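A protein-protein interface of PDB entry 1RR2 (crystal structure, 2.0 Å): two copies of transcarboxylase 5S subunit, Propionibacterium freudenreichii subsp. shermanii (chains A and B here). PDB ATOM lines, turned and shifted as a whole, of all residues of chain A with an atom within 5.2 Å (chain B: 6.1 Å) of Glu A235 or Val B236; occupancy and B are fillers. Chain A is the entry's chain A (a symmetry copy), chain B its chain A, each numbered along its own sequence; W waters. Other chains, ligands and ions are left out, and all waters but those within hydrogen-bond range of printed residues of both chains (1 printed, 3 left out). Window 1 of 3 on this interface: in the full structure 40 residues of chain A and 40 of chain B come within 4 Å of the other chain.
Water W1 lies within hydrogen-bond range of the backbone carbonyl oxygen (O) of Gly B232 and the side-chain carboxylate (OE1) of Glu A235.
Of chain B, only Gly B232, Val B233 and Val B236 come within 4 Å of Glu A235. Printed residues of chain B within 4 Å of Met A271: Pro B203 (3.2 Å), Val B233 (3.9 Å) and Val B236 (3.7 Å). Printed residues of chain B within 4 Å of Val A233: Glu B235 (3.6 Å). Of the printed residues of chain A, Gly B232 touches Glu A235 (2.7 Å) and Ser A267 (3.6 Å). Leu B238 touches none of the printed residues of chain A. Asn B263 touches none of the printed residues of chain A. The nearest residue of chain B that does not touch Glu A235 is Thr B234 (5.3 Å). The nearest printed residue of chain A that does not touch Val B233 is Val A268 (5.4 Å).
Among the printed residues, merely in contact across the chains: Met A271 with Pro B203, Ser A267 with Val B233, Ser A267 with Gly B232, Val A236 with Glu B235, Glu A235 with Val B236, Glu A235 with Val B233, Val A233 with Glu B235, Met A271 with Val B236, Val A236 with Met B239, Met A239 with Val B236 and Met A271 with Val B233.
Printed residues of chain B that touch a printed residue of chain A: Pro B203, Gly B232, Val B233, Glu B235, Val B236 and Met B239. Hydrophobic or aromatic side chains of chain B that line the printed part of chain A: Pro B203, Val B233, Val B236 and Met B239. Of the 12 printed residues of chain A, 6 touch a printed residue of chain B. Along chain A the printed residues that touch a printed residue of chain B span positions 233 to 271. Among the printed residues, 12 pairs touch across the chains.
The side-chain carboxylate of Glu A235 lies close to the backbone carbonyl oxygen of Gly B232 (2.7 Å).
The backbone carbonyl oxygen (O) of Val B233 lies within hydrogen-bond range of the side-chain hydroxyl (OG) of Ser B237 (3.5 Å). The side-chain hydroxyl (OG) of Ser A237 sits at hydrogen-bond distance from the backbone carbonyl oxygen (O) of Val A233 (3.5 Å).
Val A233 touches Glu B235, and with the chains exchanged Glu A235 touches Val B233. Glu A235 touches Val B236, and with the chains exchanged Val A236 touches Glu B235. Val A236 touches Met B239, and with the chains exchanged Met A239 touches Val B236. 8 positions are printed for both chains.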
ATOM      1  N   VAL A 233      -8.994  -7.762  -3.600  1.00  0.00           N
ATOM      2  CA  VAL A 233      -9.652  -7.912  -2.292  1.00  0.00           C
ATOM      3  C   VAL A 233      -8.829  -8.767  -1.320  1.00  0.00           C
ATOM      4  O   VAL A 233      -9.159  -8.813  -0.135  1.00  0.00           O
ATOM      5  CB  VAL A 233     -11.045  -8.645  -2.387  1.00  0.00           C
ATOM      6  CG1 VAL A 233     -11.923  -8.060  -3.506  1.00  0.00           C
ATOM      7  CG2 VAL A 233     -10.842 -10.137  -2.620  1.00  0.00           C
ATOM      8  N   THR A 234      -7.764  -9.407  -1.786  1.00  0.00           N
ATOM      9  CA  THR A 234      -7.036 -10.371  -0.947  1.00  0.00           C
ATOM     10  C   THR A 234      -6.173  -9.769   0.160  1.00  0.00           C
ATOM     11  O   THR A 234      -5.806 -10.520   1.064  1.00  0.00           O
ATOM     12  CB  THR A 234      -6.199 -11.334  -1.793  1.00  0.00           C
ATOM     13  OG1 THR A 234      -5.210 -10.605  -2.528  1.00  0.00           O
ATOM     14  CG2 THR A 234      -7.103 -12.087  -2.744  1.00  0.00           C
ATOM     15  N   GLU A 235      -5.821  -8.485   0.152  1.00  0.00           N
ATOM     16  CA  GLU A 235      -5.024  -8.032   1.302  1.00  0.00           C
ATOM     17  C   GLU A 235      -5.938  -7.995   2.524  1.00  0.00           C
ATOM     18  O   GLU A 235      -5.509  -8.153   3.683  1.00  0.00           O
ATOM     19  CB  GLU A 235      -4.421  -6.659   1.079  1.00  0.00           C
ATOM     20  CG  GLU A 235      -3.479  -6.281   2.224  1.00  0.00           C
ATOM     21  CD  GLU A 235      -2.615  -5.102   1.880  1.00  0.00           C
ATOM     22  OE1 GLU A 235      -1.840  -5.200   0.917  1.00  0.00           O
ATOM     23  OE2 GLU A 235      -2.718  -4.073   2.564  1.00  0.00           O
ATOM     24  N   VAL A 236      -7.221  -7.778   2.262  1.00  0.00           N
ATOM     25  CA  VAL A 236      -8.186  -7.773   3.368  1.00  0.00           C
ATOM     26  C   VAL A 236      -8.380  -9.219   3.808  1.00  0.00           C
ATOM     27  O   VAL A 236      -8.571  -9.494   4.989  1.00  0.00           O
ATOM     28  CB  VAL A 236      -9.540  -7.186   2.941  1.00  0.00           C
ATOM     29  CG1 VAL A 236     -10.500  -7.231   4.109  1.00  0.00           C
ATOM     30  CG2 VAL A 236      -9.365  -5.731   2.498  1.00  0.00           C
ATOM     31  N   SER A 237      -8.320 -10.144   2.847  1.00  0.00           N
ATOM     32  CA  SER A 237      -8.470 -11.572   3.159  1.00  0.00           C
ATOM     33  C   SER A 237      -7.305 -12.015   4.040  1.00  0.00           C
ATOM     34  O   SER A 237      -7.480 -12.820   4.961  1.00  0.00           O
ATOM     35  CB  SER A 237      -8.498 -12.410   1.872  1.00  0.00           C
ATOM     36  OG  SER A 237      -9.607 -12.036   1.064  1.00  0.00           O
ATOM     37  N   LEU A 238      -6.116 -11.483   3.752  1.00  0.00           N
ATOM     38  CA  LEU A 238      -4.914 -11.794   4.539  1.00  0.00           C
ATOM     39  C   LEU A 238      -5.125 -11.351   5.989  1.00  0.00           C
ATOM     40  O   LEU A 238      -4.812 -12.093   6.922  1.00  0.00           O
ATOM     41  CB  LEU A 238      -3.696 -11.085   3.959  1.00  0.00           C
ATOM     42  CG  LEU A 238      -2.720 -11.927   3.136  1.00  0.00           C
ATOM     43  CD1 LEU A 238      -3.437 -12.622   2.009  1.00  0.00           C
ATOM     44  CD2 LEU A 238      -1.609 -11.015   2.597  1.00  0.00           C
ATOM     45  N   MET A 239      -5.662 -10.147   6.181  1.00  0.00           N
ATOM     46  CA  MET A 239      -5.917  -9.661   7.545  1.00  0.00           C
ATOM     47  C   MET A 239      -6.882 -10.621   8.237  1.00  0.00           C
ATOM     48  O   MET A 239      -6.687 -10.987   9.386  1.00  0.00           O
ATOM     49  CB  MET A 239      -6.524  -8.256   7.528  1.00  0.00           C
ATOM     50  CG  MET A 239      -6.755  -7.686   8.929  1.00  0.00           C
ATOM     51  SD  MET A 239      -5.200  -7.241   9.773  1.00  0.00           S
ATOM     52  CE  MET A 239      -5.181  -8.377  11.102  1.00  0.00           C
ATOM     53  N   ASN A 263       0.020  -9.155  -2.956  1.00  0.00           N
ATOM     54  CA  ASN A 263      -0.049  -8.000  -2.051  1.00  0.00           C
ATOM     55  C   ASN A 263       1.379  -7.677  -1.620  1.00  0.00           C
ATOM     56  O   ASN A 263       2.217  -8.573  -1.529  1.00  0.00           O
ATOM     57  CB  ASN A 263      -0.933  -8.319  -0.853  1.00  0.00           C
ATOM     58  CG  ASN A 263      -2.339  -8.695  -1.271  1.00  0.00           C
ATOM     59  OD1 ASN A 263      -2.778  -9.836  -1.081  1.00  0.00           O
ATOM     60  ND2 ASN A 263      -3.048  -7.745  -1.869  1.00  0.00           N
ATOM     61  N   PRO A 264       1.666  -6.399  -1.332  1.00  0.00           N
ATOM     62  CA  PRO A 264       2.986  -5.906  -0.933  1.00  0.00           C
ATOM     63  C   PRO A 264       3.499  -6.293   0.430  1.00  0.00           C
ATOM     64  O   PRO A 264       2.812  -6.135   1.443  1.00  0.00           O
ATOM     65  CB  PRO A 264       2.855  -4.386  -1.096  1.00  0.00           C
ATOM     66  CG  PRO A 264       1.556  -4.180  -1.823  1.00  0.00           C
ATOM     67  CD  PRO A 264       0.696  -5.299  -1.349  1.00  0.00           C
ATOM     68  N   SER A 267       3.563  -3.412   2.853  1.00  0.00           N
ATOM     69  CA  SER A 267       2.176  -3.038   3.166  1.00  0.00           C
ATOM     70  C   SER A 267       1.582  -4.030   4.168  1.00  0.00           C
ATOM     71  O   SER A 267       0.958  -3.625   5.151  1.00  0.00           O
ATOM     72  CB  SER A 267       1.332  -3.007   1.885  1.00  0.00           C
ATOM     73  OG  SER A 267       1.793  -1.991   1.013  1.00  0.00           O
ATOM     74  N   VAL A 268       1.784  -5.326   3.937  1.00  0.00           N
ATOM     75  CA  VAL A 268       1.251  -6.341   4.857  1.00  0.00           C
ATOM     76  C   VAL A 268       1.946  -6.213   6.221  1.00  0.00           C
ATOM     77  O   VAL A 268       1.305  -6.394   7.262  1.00  0.00           O
ATOM     78  CB  VAL A 268       1.420  -7.766   4.261  1.00  0.00           C
ATOM     79  CG1 VAL A 268       1.136  -8.843   5.289  1.00  0.00           C
ATOM     80  CG2 VAL A 268       0.457  -7.924   3.101  1.00  0.00           C
ATOM     81  N   MET A 271       0.570  -2.733   7.993  1.00  0.00           N
ATOM     82  CA  MET A 271      -0.852  -2.688   8.368  1.00  0.00           C
ATOM     83  C   MET A 271      -1.138  -3.359   9.711  1.00  0.00           C
ATOM     84  O   MET A 271      -2.219  -3.153  10.254  1.00  0.00           O
ATOM     85  CB  MET A 271      -1.703  -3.381   7.314  1.00  0.00           C
ATOM     86  CG  MET A 271      -1.551  -4.904   7.308  1.00  0.00           C
ATOM     87  SD  MET A 271      -2.544  -5.678   6.033  1.00  0.00           S
ATOM     88  CE  MET A 271      -2.634  -7.391   6.597  1.00  0.00           C
ATOM     89  N   PRO B 203      -5.096   0.148   9.817  1.00  0.00           N
ATOM     90  CA  PRO B 203      -6.294  -0.554  10.279  1.00  0.00           C
ATOM     91  C   PRO B 203      -6.734  -0.314  11.722  1.00  0.00           C
ATOM     92  O   PRO B 203      -7.886   0.057  11.967  1.00  0.00           O
ATOM     93  CB  PRO B 203      -5.947  -2.020  10.029  1.00  0.00           C
ATOM     94  CG  PRO B 203      -5.098  -1.946   8.805  1.00  0.00           C
ATOM     95  CD  PRO B 203      -4.173  -0.796   9.164  1.00  0.00           C
ATOM     96  N   GLY B 232      -0.615   1.369   0.283  1.00  0.00           N
ATOM     97  CA  GLY B 232      -1.099   0.009   0.113  1.00  0.00           C
ATOM     98  C   GLY B 232      -1.747  -0.689   1.302  1.00  0.00           C
ATOM     99  O   GLY B 232      -2.003  -1.889   1.212  1.00  0.00           O
ATOM    100  N   VAL B 233      -2.051   0.030   2.388  1.00  0.00           N
ATOM    101  CA  VAL B 233      -2.632  -0.629   3.569  1.00  0.00           C
ATOM    102  C   VAL B 233      -4.073  -0.177   3.839  1.00  0.00           C
ATOM    103  O   VAL B 233      -4.746  -0.786   4.669  1.00  0.00           O
ATOM    104  CB  VAL B 233      -1.854  -0.298   4.901  1.00  0.00           C
ATOM    105  CG1 VAL B 233      -0.335  -0.463   4.731  1.00  0.00           C
ATOM    106  CG2 VAL B 233      -2.168   1.123   5.356  1.00  0.00           C
ATOM    107  N   THR B 234      -4.558   0.842   3.139  1.00  0.00           N
ATOM    108  CA  THR B 234      -5.867   1.426   3.467  1.00  0.00           C
ATOM    109  C   THR B 234      -7.085   0.593   3.072  1.00  0.00           C
ATOM    110  O   THR B 234      -8.162   0.880   3.595  1.00  0.00           O
ATOM    111  CB  THR B 234      -6.004   2.845   2.910  1.00  0.00           C
ATOM    112  OG1 THR B 234      -5.918   2.820   1.481  1.00  0.00           O
ATOM    113  CG2 THR B 234      -4.913   3.721   3.482  1.00  0.00           C
ATOM    114  N   GLU B 235      -6.995  -0.403   2.193  1.00  0.00           N
ATOM    115  CA  GLU B 235      -8.238  -1.147   1.939  1.00  0.00           C
ATOM    116  C   GLU B 235      -8.548  -1.983   3.177  1.00  0.00           C
ATOM    117  O   GLU B 235      -9.711  -2.303   3.491  1.00  0.00           O
ATOM    118  CB  GLU B 235      -8.127  -2.055   0.730  1.00  0.00           C
ATOM    119  CG  GLU B 235      -9.476  -2.697   0.402  1.00  0.00           C
ATOM    120  CD  GLU B 235      -9.489  -3.321  -0.963  1.00  0.00           C
ATOM    121  OE1 GLU B 235      -9.295  -2.591  -1.947  1.00  0.00           O
ATOM    122  OE2 GLU B 235      -9.682  -4.542  -1.056  1.00  0.00           O
ATOM    123  N   VAL B 236      -7.491  -2.347   3.892  1.00  0.00           N
ATOM    124  CA  VAL B 236      -7.691  -3.113   5.128  1.00  0.00           C
ATOM    125  C   VAL B 236      -8.238  -2.150   6.174  1.00  0.00           C
ATOM    126  O   VAL B 236      -9.052  -2.530   7.011  1.00  0.00           O
ATOM    127  CB  VAL B 236      -6.379  -3.726   5.638  1.00  0.00           C
ATOM    128  CG1 VAL B 236      -6.641  -4.478   6.924  1.00  0.00           C
ATOM    129  CG2 VAL B 236      -5.816  -4.700   4.600  1.00  0.00           C
ATOM    130  N   SER B 237      -7.791  -0.894   6.115  1.00  0.00           N
ATOM    131  CA  SER B 237      -8.266   0.127   7.061  1.00  0.00           C
ATOM    132  C   SER B 237      -9.759   0.356   6.837  1.00  0.00           C
ATOM    133  O   SER B 237     -10.517   0.551   7.792  1.00  0.00           O
ATOM    134  CB  SER B 237      -7.502   1.445   6.868  1.00  0.00           C
ATOM    135  OG  SER B 237      -6.115   1.252   7.118  1.00  0.00           O
ATOM    136  N   LEU B 238     -10.173   0.329   5.570  1.00  0.00           N
ATOM    137  CA  LEU B 238     -11.588   0.501   5.211  1.00  0.00           C
ATOM    138  C   LEU B 238     -12.414  -0.620   5.846  1.00  0.00           C
ATOM    139  O   LEU B 238     -13.478  -0.366   6.417  1.00  0.00           O
ATOM    140  CB  LEU B 238     -11.763   0.472   3.697  1.00  0.00           C
ATOM    141  CG  LEU B 238     -11.978   1.811   2.990  1.00  0.00           C
ATOM    142  CD1 LEU B 238     -10.860   2.768   3.313  1.00  0.00           C
ATOM    143  CD2 LEU B 238     -12.068   1.566   1.478  1.00  0.00           C
ATOM    144  N   MET B 239     -11.929  -1.855   5.754  1.00  0.00           N
ATOM    145  CA  MET B 239     -12.654  -2.982   6.360  1.00  0.00           C
ATOM    146  C   MET B 239     -12.781  -2.735   7.862  1.00  0.00           C
ATOM    147  O   MET B 239     -13.838  -2.930   8.444  1.00  0.00           O
ATOM    148  CB  MET B 239     -11.921  -4.304   6.125  1.00  0.00           C
ATOM    149  CG  MET B 239     -12.669  -5.514   6.690  1.00  0.00           C
ATOM    150  SD  MET B 239     -14.169  -5.923   5.736  1.00  0.00           S
ATOM    151  CE  MET B 239     -15.430  -5.597   6.902  1.00  0.00           C
ATOM    152  N   LYS B 240     -11.700  -2.289   8.492  1.00  0.00           N
ATOM    153  CA  LYS B 240     -11.749  -2.021   9.937  1.00  0.00           C
ATOM    154  C   LYS B 240     -12.727  -0.909  10.247  1.00  0.00           C
ATOM    155  O   LYS B 240     -13.474  -0.988  11.236  1.00  0.00           O
ATOM    156  CB  LYS B 240     -10.358  -1.667  10.468  1.00  0.00           C
ATOM    157  CG  LYS B 240      -9.479  -2.912  10.587  1.00  0.00           C
ATOM    158  CD  LYS B 240     -10.107  -3.875  11.596  1.00  0.00           C
ATOM    159  CE  LYS B 240      -9.392  -5.226  11.610  1.00  0.00           C
ATOM    160  NZ  LYS B 240     -10.124  -6.083  12.580  1.00  0.00           N
ATOM    161  N   ALA B 241     -12.727   0.133   9.418  1.00  0.00           N
ATOM    162  CA  ALA B 241     -13.636   1.266   9.649  1.00  0.00           C
ATOM    163  C   ALA B 241     -15.080   0.777   9.562  1.00  0.00           C
ATOM    164  O   ALA B 241     -15.936   1.196  10.338  1.00  0.00           O
ATOM    165  CB  ALA B 241     -13.377   2.388   8.636  1.00  0.00           C
ATOM    166  N   ASN B 263      -8.570   3.051  -3.267  1.00  0.00           N
ATOM    167  CA  ASN B 263      -8.916   1.625  -3.338  1.00  0.00           C
ATOM    168  C   ASN B 263     -10.061   1.487  -4.338  1.00  0.00           C
ATOM    169  O   ASN B 263     -10.873   2.399  -4.481  1.00  0.00           O
ATOM    170  CB  ASN B 263      -9.314   1.108  -1.963  1.00  0.00           C
ATOM    171  CG  ASN B 263      -8.204   1.290  -0.947  1.00  0.00           C
ATOM    172  OD1 ASN B 263      -8.339   2.057   0.014  1.00  0.00           O
ATOM    173  ND2 ASN B 263      -7.089   0.605  -1.168  1.00  0.00           N
HETATM  174  O   HOH W   1      -2.035  -2.877  -1.437  1.00  0.00           O
